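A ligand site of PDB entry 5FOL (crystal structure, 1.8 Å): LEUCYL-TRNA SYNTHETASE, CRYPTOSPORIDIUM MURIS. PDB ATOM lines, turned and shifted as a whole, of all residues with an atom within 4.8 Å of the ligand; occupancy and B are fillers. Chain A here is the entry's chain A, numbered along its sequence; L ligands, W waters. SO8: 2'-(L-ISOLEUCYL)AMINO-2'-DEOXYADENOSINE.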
ATOM      1  N   TYR A   8      -3.723  16.701  27.146  1.00  0.00           N
ATOM      2  CA  TYR A   8      -3.369  17.991  26.603  1.00  0.00           C
ATOM      3  C   TYR A   8      -4.608  18.597  25.942  1.00  0.00           C
ATOM      4  O   TYR A   8      -5.602  17.908  25.646  1.00  0.00           O
ATOM      5  CB  TYR A   8      -2.286  17.842  25.533  1.00  0.00           C
ATOM      6  CG  TYR A   8      -0.910  17.466  26.036  1.00  0.00           C
ATOM      7  CD1 TYR A   8      -0.530  16.118  26.203  1.00  0.00           C
ATOM      8  CD2 TYR A   8       0.022  18.433  26.356  1.00  0.00           C
ATOM      9  CE1 TYR A   8       0.732  15.759  26.668  1.00  0.00           C
ATOM     10  CE2 TYR A   8       1.288  18.082  26.810  1.00  0.00           C
ATOM     11  CZ  TYR A   8       1.626  16.738  27.010  1.00  0.00           C
ATOM     12  OH  TYR A   8       2.885  16.406  27.439  1.00  0.00           O
ATOM     13  N   ALA A  36       0.306  21.222  21.155  1.00  0.00           N
ATOM     14  CA  ALA A  36      -0.173  20.627  22.378  1.00  0.00           C
ATOM     15  C   ALA A  36       0.153  21.539  23.556  1.00  0.00           C
ATOM     16  O   ALA A  36       1.257  22.029  23.667  1.00  0.00           O
ATOM     17  CB  ALA A  36       0.452  19.257  22.589  1.00  0.00           C
ATOM     18  N   THR A  37      -0.799  21.775  24.426  1.00  0.00           N
ATOM     19  CA  THR A  37      -0.535  22.596  25.617  1.00  0.00           C
ATOM     20  C   THR A  37      -1.261  21.986  26.795  1.00  0.00           C
ATOM     21  O   THR A  37      -2.358  21.415  26.656  1.00  0.00           O
ATOM     22  CB  THR A  37      -0.961  24.091  25.413  1.00  0.00           C
ATOM     23  OG1 THR A  37      -0.554  24.877  26.547  1.00  0.00           O
ATOM     24  CG2 THR A  37      -2.440  24.244  25.302  1.00  0.00           C
ATOM     25  N   LEU A  38      -0.682  22.191  27.991  1.00  0.00           N
ATOM     26  CA  LEU A  38      -1.376  21.998  29.227  1.00  0.00           C
ATOM     27  C   LEU A  38      -2.125  23.238  29.721  1.00  0.00           C
ATOM     28  O   LEU A  38      -2.819  23.144  30.728  1.00  0.00           O
ATOM     29  CB  LEU A  38      -0.385  21.594  30.306  1.00  0.00           C
ATOM     30  CG  LEU A  38       0.410  20.323  30.078  1.00  0.00           C
ATOM     31  CD1 LEU A  38       1.270  20.111  31.320  1.00  0.00           C
ATOM     32  CD2 LEU A  38      -0.505  19.130  29.856  1.00  0.00           C
ATOM     33  N   ARG A  39      -1.952  24.388  29.058  1.00  0.00           N
ATOM     34  CA  ARG A  39      -2.486  25.677  29.574  1.00  0.00           C
ATOM     35  C   ARG A  39      -3.386  26.430  28.587  1.00  0.00           C
ATOM     36  O   ARG A  39      -3.038  27.537  28.119  1.00  0.00           O
ATOM     37  CB  ARG A  39      -1.309  26.496  30.055  1.00  0.00           C
ATOM     38  CG  ARG A  39      -0.555  25.759  31.174  1.00  0.00           C
ATOM     39  CD  ARG A  39       0.308  26.733  31.963  1.00  0.00           C
ATOM     40  NE  ARG A  39      -0.576  27.705  32.598  1.00  0.00           N
ATOM     41  CZ  ARG A  39      -0.169  28.837  33.174  1.00  0.00           C
ATOM     42  NH1 ARG A  39       1.095  29.178  33.227  1.00  0.00           N
ATOM     43  NH2 ARG A  39      -1.084  29.603  33.704  1.00  0.00           N
ATOM     44  N   THR A  42      -4.190  30.309  28.824  1.00  0.00           N
ATOM     45  CA  THR A  42      -3.222  31.338  28.458  1.00  0.00           C
ATOM     46  C   THR A  42      -3.303  31.786  26.992  1.00  0.00           C
ATOM     47  O   THR A  42      -2.424  32.527  26.569  1.00  0.00           O
ATOM     48  CB  THR A  42      -1.810  30.857  28.745  1.00  0.00           C
ATOM     49  OG1 THR A  42      -1.476  29.756  27.875  1.00  0.00           O
ATOM     50  CG2 THR A  42      -1.681  30.452  30.213  1.00  0.00           C
ATOM     51  N   MET A  43      -4.310  31.341  26.241  1.00  0.00           N
ATOM     52  CA  MET A  43      -4.383  31.609  24.813  1.00  0.00           C
ATOM     53  C   MET A  43      -4.532  33.092  24.536  1.00  0.00           C
ATOM     54  O   MET A  43      -4.102  33.565  23.498  1.00  0.00           O
ATOM     55  CB  MET A  43      -5.447  30.779  24.064  1.00  0.00           C
ATOM     56  CG  MET A  43      -5.099  29.268  23.984  1.00  0.00           C
ATOM     57  SD  MET A  43      -3.440  28.803  23.384  1.00  0.00           S
ATOM     58  CE  MET A  43      -2.541  28.558  24.897  1.00  0.00           C
ATOM     59  N   SER A 163      14.862  24.332  21.863  1.00  0.00           N
ATOM     60  CA  SER A 163      14.634  23.381  22.939  1.00  0.00           C
ATOM     61  C   SER A 163      13.460  22.414  22.687  1.00  0.00           C
ATOM     62  O   SER A 163      13.236  21.531  23.505  1.00  0.00           O
ATOM     63  CB  SER A 163      14.357  24.176  24.225  1.00  0.00           C
ATOM     64  OG  SER A 163      13.245  25.059  24.044  1.00  0.00           O
ATOM     65  N   ILE A 164      12.695  22.604  21.626  1.00  0.00           N
ATOM     66  CA  ILE A 164      11.508  21.729  21.371  1.00  0.00           C
ATOM     67  C   ILE A 164      11.926  20.258  21.245  1.00  0.00           C
ATOM     68  O   ILE A 164      12.865  19.968  20.531  1.00  0.00           O
ATOM     69  CB  ILE A 164      10.783  22.133  20.088  1.00  0.00           C
ATOM     70  CG1 ILE A 164       9.918  23.363  20.362  1.00  0.00           C
ATOM     71  CG2 ILE A 164       9.937  20.978  19.538  1.00  0.00           C
ATOM     72  CD1 ILE A 164       9.420  24.057  19.114  1.00  0.00           C
ATOM     73  N   SER A 165      11.184  19.348  21.905  1.00  0.00           N
ATOM     74  CA  SER A 165      11.347  17.924  21.703  1.00  0.00           C
ATOM     75  C   SER A 165      10.368  17.381  20.629  1.00  0.00           C
ATOM     76  O   SER A 165       9.149  17.513  20.759  1.00  0.00           O
ATOM     77  CB  SER A 165      11.134  17.190  23.022  1.00  0.00           C
ATOM     78  OG  SER A 165      11.044  15.783  22.850  1.00  0.00           O
ATOM     79  N   LYS A 168       7.595  14.914  21.955  1.00  0.00           N
ATOM     80  CA  LYS A 168       6.543  15.366  22.855  1.00  0.00           C
ATOM     81  C   LYS A 168       5.489  16.130  22.074  1.00  0.00           C
ATOM     82  O   LYS A 168       5.806  16.843  21.168  1.00  0.00           O
ATOM     83  CB  LYS A 168       7.134  16.290  23.928  1.00  0.00           C
ATOM     84  CG  LYS A 168       6.165  16.732  25.012  1.00  0.00           C
ATOM     85  CD  LYS A 168       6.834  17.702  25.965  1.00  0.00           C
ATOM     86  CE  LYS A 168       5.847  18.287  26.929  1.00  0.00           C
ATOM     87  NZ  LYS A 168       6.525  18.787  28.136  1.00  0.00           N
ATOM     88  N   GLY A 169       4.223  15.952  22.455  1.00  0.00           N
ATOM     89  CA  GLY A 169       3.124  16.658  21.807  1.00  0.00           C
ATOM     90  C   GLY A 169       3.230  16.525  20.319  1.00  0.00           C
ATOM     91  O   GLY A 169       3.506  15.419  19.797  1.00  0.00           O
ATOM     92  N   GLY A 171       5.295  18.390  18.507  1.00  0.00           N
ATOM     93  CA  GLY A 171       6.519  19.132  18.135  1.00  0.00           C
ATOM     94  C   GLY A 171       6.342  20.568  17.706  1.00  0.00           C
ATOM     95  O   GLY A 171       7.299  21.181  17.210  1.00  0.00           O
ATOM     96  N   ILE A 172       5.122  21.115  17.870  1.00  0.00           N
ATOM     97  CA  ILE A 172       4.845  22.528  17.552  1.00  0.00           C
ATOM     98  C   ILE A 172       4.199  23.131  18.777  1.00  0.00           C
ATOM     99  O   ILE A 172       3.338  22.495  19.408  1.00  0.00           O
ATOM    100  CB  ILE A 172       3.955  22.680  16.310  1.00  0.00           C
ATOM    101  CG1 ILE A 172       4.461  21.738  15.155  1.00  0.00           C
ATOM    102  CG2 ILE A 172       3.923  24.105  15.843  1.00  0.00           C
ATOM    103  CD1 ILE A 172       3.707  21.919  13.855  1.00  0.00           C
ATOM    104  N   VAL A 173       4.586  24.355  19.150  1.00  0.00           N
ATOM    105  CA  VAL A 173       4.255  24.871  20.479  1.00  0.00           C
ATOM    106  C   VAL A 173       3.834  26.325  20.311  1.00  0.00           C
ATOM    107  O   VAL A 173       4.527  27.079  19.631  1.00  0.00           O
ATOM    108  CB  VAL A 173       5.468  24.800  21.469  1.00  0.00           C
ATOM    109  CG1 VAL A 173       5.061  25.222  22.849  1.00  0.00           C
ATOM    110  CG2 VAL A 173       6.032  23.390  21.557  1.00  0.00           C
ATOM    111  N   THR A 174       2.684  26.721  20.864  1.00  0.00           N
ATOM    112  CA  THR A 174       2.347  28.131  20.793  1.00  0.00           C
ATOM    113  C   THR A 174       3.064  28.903  21.902  1.00  0.00           C
ATOM    114  O   THR A 174       3.448  28.318  22.906  1.00  0.00           O
ATOM    115  CB  THR A 174       0.816  28.393  20.778  1.00  0.00           C
ATOM    116  OG1 THR A 174       0.621  29.750  20.341  1.00  0.00           O
ATOM    117  CG2 THR A 174       0.184  28.098  22.108  1.00  0.00           C
ATOM    118  N   SER A 175       3.219  30.205  21.704  1.00  0.00           N
ATOM    119  CA  SER A 175       4.103  31.019  22.567  1.00  0.00           C
ATOM    120  C   SER A 175       3.331  32.042  23.386  1.00  0.00           C
ATOM    121  O   SER A 175       2.666  32.886  22.811  1.00  0.00           O
ATOM    122  CB  SER A 175       5.140  31.761  21.721  1.00  0.00           C
ATOM    123  OG  SER A 175       6.029  32.473  22.585  1.00  0.00           O
ATOM    124  N   VAL A 176       3.461  31.953  24.701  1.00  0.00           N
ATOM    125  CA  VAL A 176       2.843  32.910  25.637  1.00  0.00           C
ATOM    126  C   VAL A 176       3.994  33.358  26.614  1.00  0.00           C
ATOM    127  O   VAL A 176       4.124  32.869  27.759  1.00  0.00           O
ATOM    128  CB  VAL A 176       1.648  32.352  26.377  1.00  0.00           C
ATOM    129  CG1 VAL A 176       1.076  33.402  27.315  1.00  0.00           C
ATOM    130  CG2 VAL A 176       0.581  31.833  25.416  1.00  0.00           C
ATOM    131  N   ASP A 179       3.880  34.223  30.464  1.00  0.00           N
ATOM    132  CA  ASP A 179       3.611  33.250  31.491  1.00  0.00           C
ATOM    133  C   ASP A 179       4.205  31.863  31.280  1.00  0.00           C
ATOM    134  O   ASP A 179       3.843  30.936  32.026  1.00  0.00           O
ATOM    135  CB  ASP A 179       2.105  33.172  31.740  1.00  0.00           C
ATOM    136  CG  ASP A 179       1.566  34.470  32.296  1.00  0.00           C
ATOM    137  OD1 ASP A 179       1.717  34.678  33.532  1.00  0.00           O
ATOM    138  OD2 ASP A 179       1.011  35.291  31.536  1.00  0.00           O
ATOM    139  N   SER A 180       5.124  31.768  30.326  1.00  0.00           N
ATOM    140  CA  SER A 180       5.976  30.618  30.114  1.00  0.00           C
ATOM    141  C   SER A 180       7.442  31.052  30.116  1.00  0.00           C
ATOM    142  O   SER A 180       7.861  31.752  29.245  1.00  0.00           O
ATOM    143  CB  SER A 180       5.712  29.979  28.765  1.00  0.00           C
ATOM    144  OG  SER A 180       6.737  29.022  28.473  1.00  0.00           O
ATOM    145  N   ASP A 183       9.073  30.245  26.823  1.00  0.00           N
ATOM    146  CA  ASP A 183       8.706  31.162  25.727  1.00  0.00           C
ATOM    147  C   ASP A 183       9.428  32.544  25.843  1.00  0.00           C
ATOM    148  O   ASP A 183       9.821  33.147  24.822  1.00  0.00           O
ATOM    149  CB  ASP A 183       7.184  31.373  25.679  1.00  0.00           C
ATOM    150  CG  ASP A 183       6.428  30.095  25.362  1.00  0.00           C
ATOM    151  OD1 ASP A 183       7.057  29.165  24.839  1.00  0.00           O
ATOM    152  OD2 ASP A 183       5.187  30.043  25.606  1.00  0.00           O
HETATM  153  C   SO8 L   1       3.069  25.662  26.212  1.00  0.00           C
HETATM  154  N   SO8 L   1       4.278  27.576  25.388  1.00  0.00           N
HETATM  155  O   SO8 L   1       2.077  25.470  25.557  1.00  0.00           O
HETATM  156  N1  SO8 L   1       8.586  20.478  23.073  1.00  0.00           N
HETATM  157  C2  SO8 L   1       8.852  21.348  24.199  1.00  0.00           C
HETATM  158  N3  SO8 L   1       7.680  21.801  24.947  1.00  0.00           N
HETATM  159  C4  SO8 L   1       6.417  21.443  24.583  1.00  0.00           C
HETATM  160  C5  SO8 L   1       6.166  20.575  23.419  1.00  0.00           C
HETATM  161  C6  SO8 L   1       7.355  20.084  22.686  1.00  0.00           C
HETATM  162  N6  SO8 L   1       7.211  19.275  21.629  1.00  0.00           N
HETATM  163  N7  SO8 L   1       4.843  20.384  23.326  1.00  0.00           N
HETATM  164  C8  SO8 L   1       4.270  21.092  24.335  1.00  0.00           C
HETATM  165  N9  SO8 L   1       5.222  21.756  25.069  1.00  0.00           N
HETATM  166  CA  SO8 L   1       3.536  27.062  26.540  1.00  0.00           C
HETATM  167  CB  SO8 L   1       2.529  28.141  26.935  1.00  0.00           C
HETATM  168  NAI SO8 L   1       3.810  24.652  26.713  1.00  0.00           N
HETATM  169  CAJ SO8 L   1       3.600  23.245  26.391  1.00  0.00           C
HETATM  170  CAK SO8 L   1       2.980  22.464  27.530  1.00  0.00           C
HETATM  171  OAL SO8 L   1       1.979  23.150  28.261  1.00  0.00           O
HETATM  172  CAM SO8 L   1       4.233  22.159  28.357  1.00  0.00           C
HETATM  173  CAN SO8 L   1       4.023  21.087  29.407  1.00  0.00           C
HETATM  174  OAO SO8 L   1       3.529  19.920  28.774  1.00  0.00           O
HETATM  175  OAP SO8 L   1       5.237  21.793  27.384  1.00  0.00           O
HETATM  176  CAQ SO8 L   1       5.025  22.619  26.252  1.00  0.00           C
HETATM  177  CD1 SO8 L   1       1.752  29.250  29.074  1.00  0.00           C
HETATM  178  CG1 SO8 L   1       2.059  27.937  28.388  1.00  0.00           C
HETATM  179  CG2 SO8 L   1       1.377  28.303  25.933  1.00  0.00           C
HETATM  180  O   HOH W   1       2.779  24.610  30.328  1.00  0.00           O
HETATM  181  O   HOH W   2       8.550  24.425  26.079  1.00  0.00           O
HETATM  182  O   HOH W   3       6.981  26.382  25.589  1.00  0.00           O
HETATM  183  O   HOH W   4      10.953  23.673  24.786  1.00  0.00           O
HETATM  184  O   HOH W   5       4.116  23.205  32.018  1.00  0.00           O
HETATM  185  O   HOH W   6       3.356  20.093  20.955  1.00  0.00           O
HETATM  186  O   HOH W   7       3.915  17.550  30.176  1.00  0.00           O
HETATM  187  O   HOH W   8       1.588  24.737  22.882  1.00  0.00           O
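Residues that only touch the ligand: Tyr 8 (3.5 Å), Ala 36 (3.2 Å), Thr 42 (3.5 Å), Ile 164 (3.6 Å), Gly 171 (3.6 Å), Val 173 (3.4 Å), Val 176 (3.7 Å) and Asp 179 (3.99 Å).
Hydrophobic or aromatic side chains within 4 Å of the ligand: Tyr 8, Leu 38, Ile 164, Val 173 and Val 176.
14 residues have an atom within 4 Å of the ligand: Tyr 8, Ala 36, Thr 37, Leu 38, Thr 42, Ile 164, Ser 165, Lys 168, Gly 171, Val 173, Thr 174, Val 176, Asp 179 and Asp 183.
Along chain A the residues within 4 Å of the ligand span positions 8 to 183.
Water W7 bridges an oxygen (OAO) of the ligand (2.8 Å) and the side-chain hydroxyl of Tyr 8 (3.1 Å).
Water W6 lies within hydrogen-bond range of a nitrogen (N7) of the ligand, the backbone carbonyl oxygen of Ile 172 and the backbone NH of Ala 36.
Water W8 lies within hydrogen-bond range of an oxygen (O) of the ligand (2.8 Å), the backbone carbonyl oxygen of Ala 36 (2.8 Å) and the backbone NH of Thr 174 (3.0 Å).
Water W3 lies within hydrogen-bond range of the side-chain carboxylate of Asp 183 and a nitrogen (N) of the ligand.
A nitrogen (N) of the ligand is in hydrogen-bond range of the backbone carbonyl oxygen of Thr 174 (2.7 Å).
N6 of the ligand sits at hydrogen-bond distance from O of Lys 168 (2.8 Å).
The side-chain amino group (NZ) of Lys 168 sits at hydrogen-bond distance from an oxygen (OAO) of the ligand, 3.3 Å away.
An oxygen (OAL) of the ligand is in hydrogen-bond range of the backbone NH of Leu 38, 2.8 Å away.
The backbone carbonyl oxygen (O) of Ser 165 lies within hydrogen-bond range of a nitrogen (N6) of the ligand (2.8 Å).
An oxygen (O) of the ligand sits at hydrogen-bond distance from the side-chain hydroxyl (OG1) of Thr 37, at 2.9 Å.
The backbone NH (N) of Ser 165 sits at hydrogen-bond distance from a nitrogen (N1) of the ligand (3.1 Å).
The side-chain carboxylate of Asp 183 lies within salt-bridge range of a nitrogen (N) of the ligand.
OG1 of Thr 37 sits at hydrogen-bond distance from N of Arg 39 (2.9 Å).
OG1 of Thr 42 is in hydrogen-bond range of O of Arg 39 (2.7 Å).
The side-chain hydroxyl (OG) of Ser 180 sits at hydrogen-bond distance from the backbone NH (N) of Asp 183 (3.1 Å).
OD2 of Asp 183 is in hydrogen-bond range of N of Val 176 (2.7 Å).
The guanidinium group of Arg 39 lies within hydrogen-bond range of the backbone carbonyl oxygen of Asp 179, at 3.5 Å.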
